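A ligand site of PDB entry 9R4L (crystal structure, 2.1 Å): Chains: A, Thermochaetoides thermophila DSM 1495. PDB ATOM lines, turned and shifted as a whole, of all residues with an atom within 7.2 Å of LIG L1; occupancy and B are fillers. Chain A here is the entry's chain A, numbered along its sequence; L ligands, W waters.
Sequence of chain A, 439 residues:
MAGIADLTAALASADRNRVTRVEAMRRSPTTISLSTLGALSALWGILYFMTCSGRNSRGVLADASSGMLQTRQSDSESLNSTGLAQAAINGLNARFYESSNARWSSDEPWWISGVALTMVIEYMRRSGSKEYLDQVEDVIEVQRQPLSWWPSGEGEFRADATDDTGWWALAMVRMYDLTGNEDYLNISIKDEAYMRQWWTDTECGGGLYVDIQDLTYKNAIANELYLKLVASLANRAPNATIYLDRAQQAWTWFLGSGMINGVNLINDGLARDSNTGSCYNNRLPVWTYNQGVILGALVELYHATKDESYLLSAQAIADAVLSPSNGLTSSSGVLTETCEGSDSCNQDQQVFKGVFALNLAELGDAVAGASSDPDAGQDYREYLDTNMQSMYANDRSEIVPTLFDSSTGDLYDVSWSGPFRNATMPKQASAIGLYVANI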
ATOM      1  N   TRP A 111       4.054  -3.993 -20.252  1.00  0.00           N
ATOM      2  CA  TRP A 111       3.340  -4.605 -19.137  1.00  0.00           C
ATOM      3  C   TRP A 111       2.762  -5.970 -19.506  1.00  0.00           C
ATOM      4  O   TRP A 111       2.502  -6.793 -18.605  1.00  0.00           O
ATOM      5  CB  TRP A 111       2.222  -3.696 -18.640  1.00  0.00           C
ATOM      6  CG  TRP A 111       1.053  -3.499 -19.592  1.00  0.00           C
ATOM      7  CD1 TRP A 111       0.939  -2.557 -20.588  1.00  0.00           C
ATOM      8  CD2 TRP A 111      -0.191  -4.216 -19.575  1.00  0.00           C
ATOM      9  NE1 TRP A 111      -0.300  -2.652 -21.193  1.00  0.00           N
ATOM     10  CE2 TRP A 111      -1.007  -3.670 -20.600  1.00  0.00           C
ATOM     11  CE3 TRP A 111      -0.691  -5.275 -18.796  1.00  0.00           C
ATOM     12  CZ2 TRP A 111      -2.330  -4.118 -20.856  1.00  0.00           C
ATOM     13  CZ3 TRP A 111      -2.017  -5.745 -19.053  1.00  0.00           C
ATOM     14  CH2 TRP A 111      -2.812  -5.152 -20.084  1.00  0.00           C
ATOM     15  N   ASP A 163       0.193   1.210 -13.077  1.00  0.00           N
ATOM     16  CA  ASP A 163      -0.307  -0.120 -13.373  1.00  0.00           C
ATOM     17  C   ASP A 163       0.770  -1.003 -13.984  1.00  0.00           C
ATOM     18  O   ASP A 163       0.835  -2.188 -13.658  1.00  0.00           O
ATOM     19  CB  ASP A 163      -1.586  -0.097 -14.260  1.00  0.00           C
ATOM     20  CG  ASP A 163      -1.371   0.594 -15.598  1.00  0.00           C
ATOM     21  OD1 ASP A 163      -0.423   1.379 -15.746  1.00  0.00           O
ATOM     22  OD2 ASP A 163      -2.202   0.395 -16.502  1.00  0.00           O
ATOM     23  N   VAL A 210      -2.995   6.526 -12.344  1.00  0.00           N
ATOM     24  CA  VAL A 210      -2.328   5.552 -13.222  1.00  0.00           C
ATOM     25  C   VAL A 210      -1.160   6.210 -13.946  1.00  0.00           C
ATOM     26  O   VAL A 210      -0.100   5.594 -14.085  1.00  0.00           O
ATOM     27  CB  VAL A 210      -3.297   4.885 -14.237  1.00  0.00           C
ATOM     28  CG1 VAL A 210      -3.966   5.924 -15.195  1.00  0.00           C
ATOM     29  CG2 VAL A 210      -2.543   3.791 -15.059  1.00  0.00           C
ATOM     30  N   TYR A 217      -5.980  10.611 -14.044  1.00  0.00           N
ATOM     31  CA  TYR A 217      -6.882   9.461 -14.075  1.00  0.00           C
ATOM     32  C   TYR A 217      -6.633   8.531 -12.902  1.00  0.00           C
ATOM     33  O   TYR A 217      -5.559   7.897 -12.814  1.00  0.00           O
ATOM     34  CB  TYR A 217      -6.752   8.723 -15.408  1.00  0.00           C
ATOM     35  CG  TYR A 217      -7.895   7.768 -15.719  1.00  0.00           C
ATOM     36  CD1 TYR A 217      -9.157   7.929 -15.133  1.00  0.00           C
ATOM     37  CD2 TYR A 217      -7.719   6.737 -16.640  1.00  0.00           C
ATOM     38  CE1 TYR A 217     -10.222   7.065 -15.432  1.00  0.00           C
ATOM     39  CE2 TYR A 217      -8.751   5.860 -16.947  1.00  0.00           C
ATOM     40  CZ  TYR A 217     -10.012   6.046 -16.351  1.00  0.00           C
ATOM     41  OH  TYR A 217     -11.046   5.186 -16.644  1.00  0.00           O
ATOM     42  N   ASN A 219      -8.041   5.168 -12.009  1.00  0.00           N
ATOM     43  CA  ASN A 219      -8.818   4.176 -12.741  1.00  0.00           C
ATOM     44  C   ASN A 219      -8.890   2.889 -11.925  1.00  0.00           C
ATOM     45  O   ASN A 219      -8.242   2.746 -10.872  1.00  0.00           O
ATOM     46  CB  ASN A 219      -8.264   3.931 -14.151  1.00  0.00           C
ATOM     47  CG  ASN A 219      -6.879   3.280 -14.190  1.00  0.00           C
ATOM     48  OD1 ASN A 219      -6.237   3.034 -13.147  1.00  0.00           O
ATOM     49  ND2 ASN A 219      -6.413   2.965 -15.419  1.00  0.00           N
ATOM     50  N   ALA A 220      -9.734   1.963 -12.399  1.00  0.00           N
ATOM     51  CA  ALA A 220      -9.935   0.713 -11.656  1.00  0.00           C
ATOM     52  C   ALA A 220      -8.656  -0.121 -11.648  1.00  0.00           C
ATOM     53  O   ALA A 220      -8.283  -0.663 -10.614  1.00  0.00           O
ATOM     54  CB  ALA A 220     -11.095  -0.095 -12.268  1.00  0.00           C
ATOM     55  N   ILE A 221      -8.017  -0.324 -12.818  1.00  0.00           N
ATOM     56  CA  ILE A 221      -6.998  -1.374 -12.865  1.00  0.00           C
ATOM     57  C   ILE A 221      -5.799  -0.992 -11.986  1.00  0.00           C
ATOM     58  O   ILE A 221      -5.261  -1.839 -11.254  1.00  0.00           O
ATOM     59  CB  ILE A 221      -6.593  -1.687 -14.316  1.00  0.00           C
ATOM     60  CG1 ILE A 221      -5.724  -2.957 -14.366  1.00  0.00           C
ATOM     61  CG2 ILE A 221      -5.973  -0.494 -15.025  1.00  0.00           C
ATOM     62  CD1 ILE A 221      -6.411  -4.190 -13.644  1.00  0.00           C
ATOM     63  N   ALA A 222      -5.361   0.280 -12.007  1.00  0.00           N
ATOM     64  CA  ALA A 222      -4.179   0.592 -11.179  1.00  0.00           C
ATOM     65  C   ALA A 222      -4.510   0.428  -9.711  1.00  0.00           C
ATOM     66  O   ALA A 222      -3.683  -0.058  -8.927  1.00  0.00           O
ATOM     67  CB  ALA A 222      -3.683   2.010 -11.470  1.00  0.00           C
ATOM     68  N   ASP A 268     -14.652   1.509 -15.739  1.00  0.00           N
ATOM     69  CA  ASP A 268     -13.228   1.684 -15.987  1.00  0.00           C
ATOM     70  C   ASP A 268     -12.537   2.563 -14.951  1.00  0.00           C
ATOM     71  O   ASP A 268     -11.357   2.344 -14.656  1.00  0.00           O
ATOM     72  CB  ASP A 268     -12.932   2.248 -17.380  1.00  0.00           C
ATOM     73  CG  ASP A 268     -11.468   2.013 -17.754  1.00  0.00           C
ATOM     74  OD1 ASP A 268     -11.099   0.829 -17.803  1.00  0.00           O
ATOM     75  OD2 ASP A 268     -10.675   2.951 -17.958  1.00  0.00           O
ATOM     76  N   GLY A 269     -13.197   3.586 -14.435  1.00  0.00           N
ATOM     77  CA  GLY A 269     -12.512   4.459 -13.477  1.00  0.00           C
ATOM     78  C   GLY A 269     -13.370   5.609 -13.004  1.00  0.00           C
ATOM     79  O   GLY A 269     -14.607   5.581 -13.117  1.00  0.00           O
ATOM     80  N   ASN A 282     -17.059   6.874 -14.010  1.00  0.00           N
ATOM     81  CA  ASN A 282     -17.104   7.520 -15.337  1.00  0.00           C
ATOM     82  C   ASN A 282     -17.940   6.763 -16.354  1.00  0.00           C
ATOM     83  O   ASN A 282     -18.099   7.259 -17.470  1.00  0.00           O
ATOM     84  CB  ASN A 282     -15.685   7.750 -15.941  1.00  0.00           C
ATOM     85  CG  ASN A 282     -14.870   6.471 -16.115  1.00  0.00           C
ATOM     86  OD1 ASN A 282     -15.413   5.364 -16.165  1.00  0.00           O
ATOM     87  ND2 ASN A 282     -13.504   6.637 -16.204  1.00  0.00           N
ATOM     88  N   LEU A 284     -17.356   4.373 -18.209  1.00  0.00           N
ATOM     89  CA  LEU A 284     -16.624   3.716 -19.311  1.00  0.00           C
ATOM     90  C   LEU A 284     -16.768   2.197 -19.188  1.00  0.00           C
ATOM     91  O   LEU A 284     -17.234   1.689 -18.172  1.00  0.00           O
ATOM     92  CB  LEU A 284     -15.153   4.157 -19.298  1.00  0.00           C
ATOM     93  CG  LEU A 284     -14.917   5.592 -19.823  1.00  0.00           C
ATOM     94  CD1 LEU A 284     -13.389   5.901 -19.983  1.00  0.00           C
ATOM     95  CD2 LEU A 284     -15.645   5.880 -21.090  1.00  0.00           C
ATOM     96  N   PRO A 285     -16.370   1.428 -20.198  1.00  0.00           N
ATOM     97  CA  PRO A 285     -16.735   0.014 -20.250  1.00  0.00           C
ATOM     98  C   PRO A 285     -16.319  -0.837 -19.049  1.00  0.00           C
ATOM     99  O   PRO A 285     -15.395  -0.518 -18.279  1.00  0.00           O
ATOM    100  CB  PRO A 285     -16.023  -0.484 -21.512  1.00  0.00           C
ATOM    101  CG  PRO A 285     -16.035   0.748 -22.425  1.00  0.00           C
ATOM    102  CD  PRO A 285     -15.777   1.892 -21.479  1.00  0.00           C
ATOM    103  N   TRP A 287     -14.629  -4.029 -18.263  1.00  0.00           N
ATOM    104  CA  TRP A 287     -13.586  -4.868 -18.847  1.00  0.00           C
ATOM    105  C   TRP A 287     -13.359  -6.062 -17.941  1.00  0.00           C
ATOM    106  O   TRP A 287     -13.403  -5.911 -16.718  1.00  0.00           O
ATOM    107  CB  TRP A 287     -12.263  -4.092 -18.962  1.00  0.00           C
ATOM    108  CG  TRP A 287     -12.331  -2.904 -19.892  1.00  0.00           C
ATOM    109  CD1 TRP A 287     -12.197  -1.578 -19.541  1.00  0.00           C
ATOM    110  CD2 TRP A 287     -12.513  -2.927 -21.325  1.00  0.00           C
ATOM    111  NE1 TRP A 287     -12.305  -0.776 -20.663  1.00  0.00           N
ATOM    112  CE2 TRP A 287     -12.495  -1.577 -21.765  1.00  0.00           C
ATOM    113  CE3 TRP A 287     -12.713  -3.944 -22.271  1.00  0.00           C
ATOM    114  CZ2 TRP A 287     -12.642  -1.222 -23.117  1.00  0.00           C
ATOM    115  CZ3 TRP A 287     -12.911  -3.585 -23.627  1.00  0.00           C
ATOM    116  CH2 TRP A 287     -12.864  -2.243 -24.033  1.00  0.00           C
ATOM    117  N   TYR A 289     -10.782  -7.894 -17.058  1.00  0.00           N
ATOM    118  CA  TYR A 289      -9.657  -7.903 -16.093  1.00  0.00           C
ATOM    119  C   TYR A 289      -9.930  -6.993 -14.901  1.00  0.00           C
ATOM    120  O   TYR A 289      -9.356  -7.234 -13.844  1.00  0.00           O
ATOM    121  CB  TYR A 289      -8.358  -7.555 -16.841  1.00  0.00           C
ATOM    122  CG  TYR A 289      -8.048  -6.070 -17.087  1.00  0.00           C
ATOM    123  CD1 TYR A 289      -9.045  -5.168 -17.520  1.00  0.00           C
ATOM    124  CD2 TYR A 289      -6.751  -5.613 -17.092  1.00  0.00           C
ATOM    125  CE1 TYR A 289      -8.729  -3.822 -17.801  1.00  0.00           C
ATOM    126  CE2 TYR A 289      -6.423  -4.301 -17.422  1.00  0.00           C
ATOM    127  CZ  TYR A 289      -7.402  -3.402 -17.758  1.00  0.00           C
ATOM    128  OH  TYR A 289      -7.038  -2.108 -18.048  1.00  0.00           O
ATOM    129  N   ASN A 290     -10.860  -6.016 -15.023  1.00  0.00           N
ATOM    130  CA  ASN A 290     -11.249  -5.202 -13.861  1.00  0.00           C
ATOM    131  C   ASN A 290     -12.265  -5.908 -12.984  1.00  0.00           C
ATOM    132  O   ASN A 290     -12.612  -5.380 -11.915  1.00  0.00           O
ATOM    133  CB  ASN A 290     -11.824  -3.847 -14.297  1.00  0.00           C
ATOM    134  CG  ASN A 290     -10.740  -2.835 -14.585  1.00  0.00           C
ATOM    135  OD1 ASN A 290      -9.646  -2.915 -14.003  1.00  0.00           O
ATOM    136  ND2 ASN A 290     -11.025  -1.877 -15.485  1.00  0.00           N
ATOM    137  N   ASN A 346      -8.177  -4.178 -29.016  1.00  0.00           N
ATOM    138  CA  ASN A 346      -6.802  -3.763 -29.266  1.00  0.00           C
ATOM    139  C   ASN A 346      -5.815  -4.607 -28.430  1.00  0.00           C
ATOM    140  O   ASN A 346      -6.204  -5.551 -27.722  1.00  0.00           O
ATOM    141  CB  ASN A 346      -6.646  -2.252 -28.996  1.00  0.00           C
ATOM    142  CG  ASN A 346      -6.701  -1.878 -27.494  1.00  0.00           C
ATOM    143  OD1 ASN A 346      -6.682  -2.730 -26.576  1.00  0.00           O
ATOM    144  ND2 ASN A 346      -6.772  -0.582 -27.250  1.00  0.00           N
ATOM    145  N   GLN A 347      -4.522  -4.274 -28.526  1.00  0.00           N
ATOM    146  CA  GLN A 347      -3.468  -5.099 -27.932  1.00  0.00           C
ATOM    147  C   GLN A 347      -3.613  -5.216 -26.415  1.00  0.00           C
ATOM    148  O   GLN A 347      -3.293  -6.255 -25.842  1.00  0.00           O
ATOM    149  CB  GLN A 347      -2.087  -4.544 -28.337  1.00  0.00           C
ATOM    150  CG  GLN A 347      -1.719  -3.205 -27.692  1.00  0.00           C
ATOM    151  CD  GLN A 347      -2.548  -2.017 -28.172  1.00  0.00           C
ATOM    152  OE1 GLN A 347      -2.887  -1.904 -29.357  1.00  0.00           O
ATOM    153  NE2 GLN A 347      -2.869  -1.117 -27.249  1.00  0.00           N
ATOM    154  N   ASP A 348      -4.157  -4.178 -25.762  1.00  0.00           N
ATOM    155  CA  ASP A 348      -4.431  -4.272 -24.324  1.00  0.00           C
ATOM    156  C   ASP A 348      -5.576  -5.236 -24.051  1.00  0.00           C
ATOM    157  O   ASP A 348      -5.427  -6.231 -23.305  1.00  0.00           O
ATOM    158  CB  ASP A 348      -4.759  -2.877 -23.750  1.00  0.00           C
ATOM    159  CG  ASP A 348      -3.625  -1.864 -23.935  1.00  0.00           C
ATOM    160  OD1 ASP A 348      -2.468  -2.295 -24.034  1.00  0.00           O
ATOM    161  OD2 ASP A 348      -3.875  -0.647 -23.961  1.00  0.00           O
ATOM    162  N   GLN A 349      -6.721  -4.973 -24.665  1.00  0.00           N
ATOM    163  CA  GLN A 349      -7.946  -5.713 -24.405  1.00  0.00           C
ATOM    164  C   GLN A 349      -7.801  -7.183 -24.776  1.00  0.00           C
ATOM    165  O   GLN A 349      -8.514  -8.037 -24.228  1.00  0.00           O
ATOM    166  CB  GLN A 349      -9.120  -5.025 -25.193  1.00  0.00           C
ATOM    167  CG  GLN A 349      -9.388  -3.582 -24.705  1.00  0.00           C
ATOM    168  CD  GLN A 349      -9.605  -2.550 -25.850  1.00  0.00           C
ATOM    169  OE1 GLN A 349      -9.684  -2.911 -26.995  1.00  0.00           O
ATOM    170  NE2 GLN A 349      -9.683  -1.267 -25.499  1.00  0.00           N
ATOM    171  N   PHE A 352      -7.131  -9.359 -21.622  1.00  0.00           N
ATOM    172  CA  PHE A 352      -7.927  -9.166 -20.409  1.00  0.00           C
ATOM    173  C   PHE A 352      -8.525 -10.472 -19.857  1.00  0.00           C
ATOM    174  O   PHE A 352      -8.541 -10.693 -18.644  1.00  0.00           O
ATOM    175  CB  PHE A 352      -9.035  -8.156 -20.684  1.00  0.00           C
ATOM    176  CG  PHE A 352      -8.586  -6.722 -20.801  1.00  0.00           C
ATOM    177  CD1 PHE A 352      -7.244  -6.365 -20.589  1.00  0.00           C
ATOM    178  CD2 PHE A 352      -9.524  -5.725 -21.140  1.00  0.00           C
ATOM    179  CE1 PHE A 352      -6.832  -5.038 -20.723  1.00  0.00           C
ATOM    180  CE2 PHE A 352      -9.153  -4.383 -21.268  1.00  0.00           C
ATOM    181  CZ  PHE A 352      -7.785  -4.028 -21.071  1.00  0.00           C
HETATM  182  C1  LIG L   1      -6.228   2.298 -20.962  1.00  0.00           C
HETATM  183  C2  LIG L   1      -6.738   2.777 -19.548  1.00  0.00           C
HETATM  184  C3  LIG L   1      -7.450   1.648 -18.723  1.00  0.00           C
HETATM  185  C4  LIG L   1      -8.455   0.834 -19.598  1.00  0.00           C
HETATM  186  C5  LIG L   1      -7.823   0.387 -20.881  1.00  0.00           C
HETATM  187  C6  LIG L   1      -8.932  -0.250 -21.821  1.00  0.00           C
HETATM  188  O1  LIG L   1      -5.019   1.645 -20.807  1.00  0.00           O
HETATM  189  O2  LIG L   1      -7.770   3.714 -19.803  1.00  0.00           O
HETATM  190  O3  LIG L   1      -8.208   2.209 -17.571  1.00  0.00           O
HETATM  191  O4  LIG L   1      -8.997  -0.368 -18.932  1.00  0.00           O
HETATM  192  O5  LIG L   1      -7.225   1.491 -21.577  1.00  0.00           O
HETATM  193  O6  LIG L   1      -8.275  -0.862 -22.930  1.00  0.00           O
HETATM  194  C1  LG2 L   2     -10.198   8.928 -19.848  1.00  0.00           C
HETATM  195  C2  LG2 L   2      -8.732   8.941 -19.260  1.00  0.00           C
HETATM  196  C3  LG2 L   2      -8.402  10.254 -18.397  1.00  0.00           C
HETATM  197  C4  LG2 L   2      -9.652  10.969 -17.876  1.00  0.00           C
HETATM  198  C5  LG2 L   2     -10.721   9.929 -17.617  1.00  0.00           C
HETATM  199  C6  LG2 L   2     -11.879  10.440 -16.704  1.00  0.00           C
HETATM  200  O1  LG2 L   2     -10.411   7.564 -20.338  1.00  0.00           O
HETATM  201  O2  LG2 L   2      -7.722   8.780 -20.296  1.00  0.00           O
HETATM  202  O3  LG2 L   2      -7.481  11.169 -19.045  1.00  0.00           O
HETATM  203  O4  LG2 L   2      -9.403  11.655 -16.671  1.00  0.00           O
HETATM  204  O5  LG2 L   2     -11.218   9.425 -18.938  1.00  0.00           O
HETATM  205  O6  LG2 L   2     -12.779   9.335 -16.529  1.00  0.00           O
HETATM  206  O   HOH W   1      -3.152  -0.006 -20.874  1.00  0.00           O
HETATM  207  O   HOH W   2      -6.514   6.229 -20.177  1.00  0.00           O
HETATM  208  O   HOH W   3     -10.179   4.065 -20.603  1.00  0.00           O
HETATM  209  O   HOH W   4      -9.183   0.524 -15.507  1.00  0.00           O
HETATM  210  O   HOH W   5      -4.576  -1.334 -19.082  1.00  0.00           O
HETATM  211  O   HOH W   6      -8.645   2.978 -23.555  1.00  0.00           O
HETATM  212  O   HOH W   7      -6.232   0.578 -24.455  1.00  0.00           O
HETATM  213  O   HOH W   8      -4.236   1.655 -17.532  1.00  0.00           O
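Water W1 lies within hydrogen-bond range of an oxygen (O1) of LIG L1 (2.5 Å) and the side-chain carboxylate (OD2) of Asp 348 (3.2 Å). Water W3 lies within hydrogen-bond range of O2 of LIG L1 (2.6 Å) and OD2 of Asp 268 (2.9 Å). Water W2 lies within hydrogen-bond range of O2 of LG2 L2 (2.8 Å) and O2 of LIG L1 (2.8 Å). Water W7 lies within hydrogen-bond range of the side-chain carboxylate (OD2) of Asp 348 (2.7 Å), an oxygen (O6) of LIG L1 (2.9 Å) and the side-chain amide nitrogen (ND2) of Asn 346 (3.1 Å). Water W8 lies within hydrogen-bond range of OD2 of Asp 163 (2.6 Å), ND2 of Asn 219 (3.3 Å) and O1 of LIG L1 (3.4 Å). Water W5 bridges the side-chain hydroxyl (OH) of Tyr 289 and an oxygen (O1) of LIG L1.
The side-chain carboxylate of Asp 268 sits close to the indole nitrogen of Trp 287 (3.5 Å). OD2 of Asp 268 is in hydrogen-bond range of OH of Tyr 217, at 2.6 Å. The backbone carbonyl oxygen (O) of Asp 268 sits at hydrogen-bond distance from the backbone NH (N) of Ala 220, at 2.8 Å. O of Pro 285 is in hydrogen-bond range of N of Asp 268 (3.3 Å). The side-chain amide oxygen (OD1) of Asn 219 sits at hydrogen-bond distance from the backbone NH (N) of Ala 222 (3.1 Å). OE1 of Gln 349 is in hydrogen-bond range of N of Asn 346. O of Tyr 217 lies within hydrogen-bond range of N of Val 210 (2.9 Å). The backbone NH of Gly 269 sits at hydrogen-bond distance from the side-chain hydroxyl of Tyr 217, at 3.5 Å.
The side-chain carboxylate (OD2) of Asp 268 is in hydrogen-bond range of an oxygen (O3) of LIG L1. OH of Tyr 289 lies within hydrogen-bond range of O4 of LIG L1, 2.8 Å away. An oxygen (O3) of LIG L1 lies within hydrogen-bond range of the side-chain amide nitrogen (ND2) of Asn 219, at 2.9 Å. The side-chain amide nitrogen of Gln 349 lies within hydrogen-bond range of an oxygen (O6) of LIG L1 (3.0 Å). The side-chain amide nitrogen (ND2) of Asn 282 is in hydrogen-bond range of an oxygen (O6) of LG2 L2 (2.8 Å).
Merely in contact with LIG L1: Trp 287, Phe 352 and Tyr 217. Hydrophobic or aromatic side chains within 4 Å of LIG L1: Tyr 217, Trp 287, Tyr 289 and Phe 352. Of the 21 residues printed, 7 come within 4 Å of LIG L1.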
